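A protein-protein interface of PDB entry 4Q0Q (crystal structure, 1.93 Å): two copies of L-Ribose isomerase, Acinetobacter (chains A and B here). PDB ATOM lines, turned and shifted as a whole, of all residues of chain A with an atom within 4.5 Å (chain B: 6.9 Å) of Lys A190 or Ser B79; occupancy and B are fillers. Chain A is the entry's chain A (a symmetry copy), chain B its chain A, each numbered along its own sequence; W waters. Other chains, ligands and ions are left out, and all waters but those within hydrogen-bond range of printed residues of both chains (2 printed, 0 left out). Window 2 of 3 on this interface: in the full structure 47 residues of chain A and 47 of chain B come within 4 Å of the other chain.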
ATOM      1  N   TYR A 126     -12.685  25.018  17.858  1.00  0.00           N
ATOM      2  CA  TYR A 126     -11.725  25.100  18.954  1.00  0.00           C
ATOM      3  C   TYR A 126     -12.292  25.631  20.259  1.00  0.00           C
ATOM      4  O   TYR A 126     -13.119  26.546  20.279  1.00  0.00           O
ATOM      5  CB  TYR A 126     -10.537  25.991  18.570  1.00  0.00           C
ATOM      6  CG  TYR A 126      -9.993  25.752  17.185  1.00  0.00           C
ATOM      7  CD1 TYR A 126      -9.663  24.470  16.757  1.00  0.00           C
ATOM      8  CD2 TYR A 126      -9.815  26.813  16.297  1.00  0.00           C
ATOM      9  CE1 TYR A 126      -9.170  24.246  15.470  1.00  0.00           C
ATOM     10  CE2 TYR A 126      -9.324  26.606  15.016  1.00  0.00           C
ATOM     11  CZ  TYR A 126      -9.002  25.320  14.606  1.00  0.00           C
ATOM     12  OH  TYR A 126      -8.511  25.116  13.338  1.00  0.00           O
ATOM     13  N   GLU A 127     -11.808  25.045  21.347  1.00  0.00           N
ATOM     14  CA  GLU A 127     -12.176  25.425  22.696  1.00  0.00           C
ATOM     15  C   GLU A 127     -10.866  25.438  23.476  1.00  0.00           C
ATOM     16  O   GLU A 127     -10.285  24.381  23.728  1.00  0.00           O
ATOM     17  CB  GLU A 127     -13.127  24.393  23.303  1.00  0.00           C
ATOM     18  CG  GLU A 127     -13.521  24.662  24.749  1.00  0.00           C
ATOM     19  CD  GLU A 127     -14.329  23.519  25.355  1.00  0.00           C
ATOM     20  OE1 GLU A 127     -15.187  22.955  24.653  1.00  0.00           O
ATOM     21  OE2 GLU A 127     -14.114  23.195  26.539  1.00  0.00           O
ATOM     22  N   ASP A 188     -14.140  31.622  25.720  1.00  0.00           N
ATOM     23  CA  ASP A 188     -14.657  32.269  24.518  1.00  0.00           C
ATOM     24  C   ASP A 188     -15.676  31.393  23.808  1.00  0.00           C
ATOM     25  O   ASP A 188     -15.801  30.201  24.086  1.00  0.00           O
ATOM     26  CB  ASP A 188     -13.531  32.576  23.520  1.00  0.00           C
ATOM     27  CG  ASP A 188     -12.682  33.758  23.933  1.00  0.00           C
ATOM     28  OD1 ASP A 188     -13.134  34.552  24.779  1.00  0.00           O
ATOM     29  OD2 ASP A 188     -11.565  33.902  23.396  1.00  0.00           O
ATOM     30  N   PRO A 189     -16.449  31.988  22.889  1.00  0.00           N
ATOM     31  CA  PRO A 189     -17.432  31.190  22.159  1.00  0.00           C
ATOM     32  C   PRO A 189     -16.627  30.179  21.335  1.00  0.00           C
ATOM     33  O   PRO A 189     -15.453  30.416  21.031  1.00  0.00           O
ATOM     34  CB  PRO A 189     -18.113  32.223  21.258  1.00  0.00           C
ATOM     35  CG  PRO A 189     -17.991  33.494  22.033  1.00  0.00           C
ATOM     36  CD  PRO A 189     -16.589  33.422  22.584  1.00  0.00           C
ATOM     37  N   LYS A 190     -17.237  29.051  20.989  1.00  0.00           N
ATOM     38  CA  LYS A 190     -16.552  28.045  20.174  1.00  0.00           C
ATOM     39  C   LYS A 190     -16.173  28.702  18.845  1.00  0.00           C
ATOM     40  O   LYS A 190     -16.955  29.466  18.293  1.00  0.00           O
ATOM     41  CB  LYS A 190     -17.489  26.866  19.904  1.00  0.00           C
ATOM     42  CG  LYS A 190     -17.740  25.949  21.091  1.00  0.00           C
ATOM     43  CD  LYS A 190     -16.645  24.904  21.222  1.00  0.00           C
ATOM     44  CE  LYS A 190     -17.106  23.735  22.077  1.00  0.00           C
ATOM     45  NZ  LYS A 190     -16.064  22.678  22.248  1.00  0.00           N
ATOM     46  N   PHE A 191     -14.982  28.412  18.334  1.00  0.00           N
ATOM     47  CA  PHE A 191     -14.551  28.991  17.067  1.00  0.00           C
ATOM     48  C   PHE A 191     -14.531  27.913  15.983  1.00  0.00           C
ATOM     49  O   PHE A 191     -13.856  26.896  16.125  1.00  0.00           O
ATOM     50  CB  PHE A 191     -13.150  29.599  17.207  1.00  0.00           C
ATOM     51  CG  PHE A 191     -12.716  30.397  16.007  1.00  0.00           C
ATOM     52  CD1 PHE A 191     -13.211  31.680  15.790  1.00  0.00           C
ATOM     53  CD2 PHE A 191     -11.823  29.860  15.083  1.00  0.00           C
ATOM     54  CE1 PHE A 191     -12.821  32.418  14.663  1.00  0.00           C
ATOM     55  CE2 PHE A 191     -11.429  30.585  13.958  1.00  0.00           C
ATOM     56  CZ  PHE A 191     -11.930  31.867  13.748  1.00  0.00           C
ATOM     57  N   VAL A 192     -15.257  28.143  14.893  1.00  0.00           N
ATOM     58  CA  VAL A 192     -15.335  27.174  13.801  1.00  0.00           C
ATOM     59  C   VAL A 192     -14.353  27.411  12.638  1.00  0.00           C
ATOM     60  O   VAL A 192     -14.202  28.526  12.144  1.00  0.00           O
ATOM     61  CB  VAL A 192     -16.790  27.120  13.238  1.00  0.00           C
ATOM     62  CG1 VAL A 192     -16.870  26.206  12.016  1.00  0.00           C
ATOM     63  CG2 VAL A 192     -17.743  26.629  14.322  1.00  0.00           C
ATOM     64  N   VAL A 216     -13.201  19.835  18.421  1.00  0.00           N
ATOM     65  CA  VAL A 216     -14.385  19.022  18.179  1.00  0.00           C
ATOM     66  C   VAL A 216     -14.625  19.229  16.690  1.00  0.00           C
ATOM     67  O   VAL A 216     -14.884  20.352  16.248  1.00  0.00           O
ATOM     68  CB  VAL A 216     -15.608  19.506  18.990  1.00  0.00           C
ATOM     69  CG1 VAL A 216     -16.865  18.823  18.476  1.00  0.00           C
ATOM     70  CG2 VAL A 216     -15.420  19.172  20.471  1.00  0.00           C
ATOM     71  N   TYR B  38     -16.231  24.456  31.424  1.00  0.00           N
ATOM     72  CA  TYR B  38     -16.992  24.393  30.182  1.00  0.00           C
ATOM     73  C   TYR B  38     -17.216  25.847  29.774  1.00  0.00           C
ATOM     74  O   TYR B  38     -17.572  26.678  30.603  1.00  0.00           O
ATOM     75  CB  TYR B  38     -18.339  23.699  30.373  1.00  0.00           C
ATOM     76  CG  TYR B  38     -18.979  23.320  29.056  1.00  0.00           C
ATOM     77  CD1 TYR B  38     -18.544  22.194  28.343  1.00  0.00           C
ATOM     78  CD2 TYR B  38     -19.999  24.095  28.507  1.00  0.00           C
ATOM     79  CE1 TYR B  38     -19.114  21.856  27.118  1.00  0.00           C
ATOM     80  CE2 TYR B  38     -20.575  23.766  27.279  1.00  0.00           C
ATOM     81  CZ  TYR B  38     -20.131  22.647  26.591  1.00  0.00           C
ATOM     82  OH  TYR B  38     -20.716  22.315  25.385  1.00  0.00           O
ATOM     83  N   PRO B  39     -17.016  26.170  28.490  1.00  0.00           N
ATOM     84  CA  PRO B  39     -17.196  27.542  27.998  1.00  0.00           C
ATOM     85  C   PRO B  39     -18.644  28.005  27.890  1.00  0.00           C
ATOM     86  O   PRO B  39     -19.237  27.972  26.808  1.00  0.00           O
ATOM     87  CB  PRO B  39     -16.505  27.505  26.645  1.00  0.00           C
ATOM     88  CG  PRO B  39     -16.832  26.111  26.159  1.00  0.00           C
ATOM     89  CD  PRO B  39     -16.589  25.269  27.401  1.00  0.00           C
ATOM     90  N   ILE B  40     -19.213  28.435  29.012  1.00  0.00           N
ATOM     91  CA  ILE B  40     -20.592  28.910  29.016  1.00  0.00           C
ATOM     92  C   ILE B  40     -20.614  30.420  28.852  1.00  0.00           C
ATOM     93  O   ILE B  40     -20.069  31.153  29.679  1.00  0.00           O
ATOM     94  CB  ILE B  40     -21.321  28.522  30.324  1.00  0.00           C
ATOM     95  CG1 ILE B  40     -21.447  26.996  30.410  1.00  0.00           C
ATOM     96  CG2 ILE B  40     -22.718  29.157  30.358  1.00  0.00           C
ATOM     97  CD1 ILE B  40     -22.000  26.487  31.713  1.00  0.00           C
ATOM     98  N   THR B  41     -21.222  30.882  27.766  1.00  0.00           N
ATOM     99  CA  THR B  41     -21.328  32.313  27.497  1.00  0.00           C
ATOM    100  C   THR B  41     -22.693  32.794  27.987  1.00  0.00           C
ATOM    101  O   THR B  41     -23.544  31.983  28.347  1.00  0.00           O
ATOM    102  CB  THR B  41     -21.179  32.618  25.986  1.00  0.00           C
ATOM    103  OG1 THR B  41     -22.187  31.919  25.250  1.00  0.00           O
ATOM    104  CG2 THR B  41     -19.806  32.178  25.486  1.00  0.00           C
ATOM    105  N   MET B  44     -25.985  31.548  26.421  1.00  0.00           N
ATOM    106  CA  MET B  44     -26.286  30.145  26.688  1.00  0.00           C
ATOM    107  C   MET B  44     -27.146  29.999  27.942  1.00  0.00           C
ATOM    108  O   MET B  44     -27.860  29.014  28.111  1.00  0.00           O
ATOM    109  CB  MET B  44     -24.978  29.351  26.836  1.00  0.00           C
ATOM    110  CG  MET B  44     -24.222  29.181  25.521  1.00  0.00           C
ATOM    111  SD  MET B  44     -22.512  28.607  25.703  1.00  0.00           S
ATOM    112  CE  MET B  44     -22.736  27.134  26.672  1.00  0.00           C
ATOM    113  N   PHE B  77     -26.652  23.258  28.247  1.00  0.00           N
ATOM    114  CA  PHE B  77     -25.997  24.477  27.804  1.00  0.00           C
ATOM    115  C   PHE B  77     -25.309  24.122  26.497  1.00  0.00           C
ATOM    116  O   PHE B  77     -24.328  23.384  26.489  1.00  0.00           O
ATOM    117  CB  PHE B  77     -24.963  24.938  28.831  1.00  0.00           C
ATOM    118  CG  PHE B  77     -25.565  25.422  30.124  1.00  0.00           C
ATOM    119  CD1 PHE B  77     -26.435  26.510  30.134  1.00  0.00           C
ATOM    120  CD2 PHE B  77     -25.237  24.815  31.330  1.00  0.00           C
ATOM    121  CE1 PHE B  77     -26.968  26.990  31.335  1.00  0.00           C
ATOM    122  CE2 PHE B  77     -25.762  25.283  32.534  1.00  0.00           C
ATOM    123  CZ  PHE B  77     -26.630  26.376  32.535  1.00  0.00           C
ATOM    124  N   GLU B  78     -25.845  24.640  25.397  1.00  0.00           N
ATOM    125  CA  GLU B  78     -25.308  24.371  24.071  1.00  0.00           C
ATOM    126  C   GLU B  78     -24.250  25.395  23.662  1.00  0.00           C
ATOM    127  O   GLU B  78     -24.562  26.570  23.450  1.00  0.00           O
ATOM    128  CB  GLU B  78     -26.466  24.361  23.070  1.00  0.00           C
ATOM    129  CG  GLU B  78     -26.101  24.087  21.634  1.00  0.00           C
ATOM    130  CD  GLU B  78     -27.327  24.028  20.739  1.00  0.00           C
ATOM    131  OE1 GLU B  78     -27.922  22.936  20.599  1.00  0.00           O
ATOM    132  OE2 GLU B  78     -27.705  25.082  20.185  1.00  0.00           O
ATOM    133  N   SER B  79     -22.998  24.954  23.558  1.00  0.00           N
ATOM    134  CA  SER B  79     -21.918  25.860  23.168  1.00  0.00           C
ATOM    135  C   SER B  79     -21.678  25.831  21.664  1.00  0.00           C
ATOM    136  O   SER B  79     -21.074  26.747  21.095  1.00  0.00           O
ATOM    137  CB  SER B  79     -20.615  25.486  23.885  1.00  0.00           C
ATOM    138  OG  SER B  79     -20.133  24.225  23.449  1.00  0.00           O
ATOM    139  N   LEU B  80     -22.150  24.771  21.017  1.00  0.00           N
ATOM    140  CA  LEU B  80     -21.953  24.628  19.590  1.00  0.00           C
ATOM    141  C   LEU B  80     -23.023  23.773  18.913  1.00  0.00           C
ATOM    142  O   LEU B  80     -23.379  22.697  19.398  1.00  0.00           O
ATOM    143  CB  LEU B  80     -20.576  24.007  19.331  1.00  0.00           C
ATOM    144  CG  LEU B  80     -20.174  23.812  17.866  1.00  0.00           C
ATOM    145  CD1 LEU B  80     -19.777  25.150  17.252  1.00  0.00           C
ATOM    146  CD2 LEU B  80     -19.019  22.825  17.785  1.00  0.00           C
ATOM    147  N   ASN B  81     -23.535  24.281  17.797  1.00  0.00           N
ATOM    148  CA  ASN B  81     -24.521  23.591  16.975  1.00  0.00           C
ATOM    149  C   ASN B  81     -24.276  24.146  15.578  1.00  0.00           C
ATOM    150  O   ASN B  81     -24.992  25.019  15.080  1.00  0.00           O
ATOM    151  CB  ASN B  81     -25.953  23.875  17.445  1.00  0.00           C
ATOM    152  CG  ASN B  81     -26.948  22.863  16.898  1.00  0.00           C
ATOM    153  OD1 ASN B  81     -26.609  21.697  16.695  1.00  0.00           O
ATOM    154  ND2 ASN B  81     -28.183  23.297  16.677  1.00  0.00           N
ATOM    155  N   CYS B 102     -22.318  19.395  17.207  1.00  0.00           N
ATOM    156  CA  CYS B 102     -23.032  19.933  18.360  1.00  0.00           C
ATOM    157  C   CYS B 102     -22.308  19.573  19.659  1.00  0.00           C
ATOM    158  O   CYS B 102     -22.020  18.401  19.916  1.00  0.00           O
ATOM    159  CB  CYS B 102     -24.470  19.392  18.392  1.00  0.00           C
ATOM    160  SG  CYS B 102     -25.547  20.131  19.668  1.00  0.00           S
ATOM    161  N   ASP B 103     -22.012  20.591  20.468  1.00  0.00           N
ATOM    162  CA  ASP B 103     -21.323  20.408  21.748  1.00  0.00           C
ATOM    163  C   ASP B 103     -22.195  21.043  22.826  1.00  0.00           C
ATOM    164  O   ASP B 103     -22.629  22.183  22.682  1.00  0.00           O
ATOM    165  CB  ASP B 103     -19.961  21.117  21.716  1.00  0.00           C
ATOM    166  CG  ASP B 103     -19.017  20.638  22.807  1.00  0.00           C
ATOM    167  OD1 ASP B 103     -19.458  20.493  23.963  1.00  0.00           O
ATOM    168  OD2 ASP B 103     -17.819  20.415  22.506  1.00  0.00           O
ATOM    169  N   LYS B 104     -22.473  20.313  23.895  1.00  0.00           N
ATOM    170  CA  LYS B 104     -23.286  20.865  24.960  1.00  0.00           C
ATOM    171  C   LYS B 104     -22.986  20.196  26.287  1.00  0.00           C
ATOM    172  O   LYS B 104     -22.505  19.065  26.335  1.00  0.00           O
ATOM    173  CB  LYS B 104     -24.777  20.723  24.631  1.00  0.00           C
ATOM    174  CG  LYS B 104     -25.327  19.310  24.759  1.00  0.00           C
ATOM    175  CD  LYS B 104     -25.853  18.788  23.421  1.00  0.00           C
ATOM    176  CE  LYS B 104     -24.728  18.634  22.406  1.00  0.00           C
ATOM    177  NZ  LYS B 104     -25.190  18.068  21.101  1.00  0.00           N
ATOM    178  N   LEU B 105     -23.256  20.921  27.368  1.00  0.00           N
ATOM    179  CA  LEU B 105     -23.048  20.403  28.705  1.00  0.00           C
ATOM    180  C   LEU B 105     -24.434  20.066  29.243  1.00  0.00           C
ATOM    181  O   LEU B 105     -25.346  20.892  29.178  1.00  0.00           O
ATOM    182  CB  LEU B 105     -22.394  21.461  29.589  1.00  0.00           C
ATOM    183  CG  LEU B 105     -21.903  20.916  30.927  1.00  0.00           C
ATOM    184  CD1 LEU B 105     -20.754  19.940  30.668  1.00  0.00           C
ATOM    185  CD2 LEU B 105     -21.457  22.062  31.833  1.00  0.00           C
ATOM    186  N   ARG B 214     -20.664  15.982  29.057  1.00  0.00           N
ATOM    187  CA  ARG B 214     -20.475  16.696  27.816  1.00  0.00           C
ATOM    188  C   ARG B 214     -20.897  15.810  26.646  1.00  0.00           C
ATOM    189  O   ARG B 214     -20.397  14.693  26.477  1.00  0.00           O
ATOM    190  CB  ARG B 214     -19.006  17.098  27.621  1.00  0.00           C
ATOM    191  CG  ARG B 214     -18.761  17.766  26.255  1.00  0.00           C
ATOM    192  CD  ARG B 214     -17.278  17.937  25.942  1.00  0.00           C
ATOM    193  NE  ARG B 214     -16.602  18.790  26.916  1.00  0.00           N
ATOM    194  CZ  ARG B 214     -16.158  20.018  26.659  1.00  0.00           C
ATOM    195  NH1 ARG B 214     -15.558  20.712  27.615  1.00  0.00           N
ATOM    196  NH2 ARG B 214     -16.306  20.547  25.450  1.00  0.00           N
ATOM    197  N   VAL B 216     -21.011  15.324  22.611  1.00  0.00           N
ATOM    198  CA  VAL B 216     -20.415  15.765  21.358  1.00  0.00           C
ATOM    199  C   VAL B 216     -21.166  14.933  20.328  1.00  0.00           C
ATOM    200  O   VAL B 216     -21.078  13.703  20.334  1.00  0.00           O
ATOM    201  CB  VAL B 216     -18.901  15.465  21.287  1.00  0.00           C
ATOM    202  CG1 VAL B 216     -18.405  15.668  19.865  1.00  0.00           C
ATOM    203  CG2 VAL B 216     -18.137  16.400  22.227  1.00  0.00           C
HETATM  204  O   HOH W   1     -18.434  28.600  24.245  1.00  0.00           O
HETATM  205  O   HOH W   2     -19.794  28.885  22.055  1.00  0.00           O
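The side-chain carboxylate (OD1) of Asp B103 lies within hydrogen-bond range of the side-chain hydroxyl (OH) of Tyr B38 (2.6 Å).
OE1 of Glu A127 is in salt-bridge range of NZ of Lys A190 (2.6 Å).
O of Leu B80 sits close to SG of Cys B102.
The backbone NH of Ser B79 lies within hydrogen-bond range of the backbone carbonyl oxygen of Asp B103 (2.9 Å).
The side-chain hydroxyl of Ser B79 lies within hydrogen-bond range of the side-chain hydroxyl of Tyr B38 (2.8 Å).
The guanidinium group (NH2) of Arg B214 lies within salt-bridge range of the side-chain carboxylate (OD2) of Asp B103 (3.3 Å).
The side-chain carboxylate (OE1) of Glu A127 lies within salt-bridge range of the guanidinium group (NH2) of Arg B214 (2.8 Å).
The side-chain amino group (NZ) of Lys A190 is in salt-bridge range of the side-chain carboxylate (OD2) of Asp B103, 2.9 Å away.
Water W2 bridges the backbone carbonyl oxygen (O) of Ser B79 (2.7 Å) and the backbone NH (N) of Lys A190 (2.8 Å).
Water W1 lies within hydrogen-bond range of the backbone carbonyl oxygen (O) of Pro B39 (2.8 Å), the backbone carbonyl oxygen (O) of Asp A188 (3.1 Å) and the backbone NH (N) of Lys A190 (3.5 Å).
Val B216 touches its own counterpart, Val A216.
Of the 10 pairs that touch across the chains among the printed residues, 1 has its exchanged pair printed and touching as well.
Printed residues of chain A that touch a printed residue of chain B: Glu A127, Asp A188, Lys A190, Val A192 and Val A216.
Among the printed residues, 10 pairs touch across the chains.
Glu A127 touches Pro B39 (OE2 to CD, 3.3 Å).
CB of Pro B39 touches O of Asp A188 (3.8 Å).
Ser B79 touches Lys A190.
Lys A190 touches Leu B80 (CG to CB, 3.9 Å).
NZ of Lys A190 touches NH2 of Arg B214, 3.9 Å away.
Val A192 touches Leu B80.
Val A216 touches Asp B103.
CG1 of Val A216 touches CG1 of Val B216, at 3.8 Å.
Of the printed residues of chain B, Glu A127 touches Pro B39 (3.3 Å) and Arg B214 (2.8 Å).
Of the printed residues of chain B, Val A192 touches Leu B80.
Printed residues of chain B within 4 Å of Val A216: Asp B103 (3.4 Å) and Val B216 (3.8 Å).
Of the printed residues of chain A, Pro B39 touches Glu A127 and Asp A188.
Ile B40 touches none of the printed residues of chain A.
Ser B79 touches just one residue of chain A: Lys A190 (3.4 Å).
Printed residues of chain A within 4 Å of Leu B80: Lys A190 and Val A192.
The nearest residue of chain B that does not touch Lys A190 is Pro B39 (4.7 Å).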
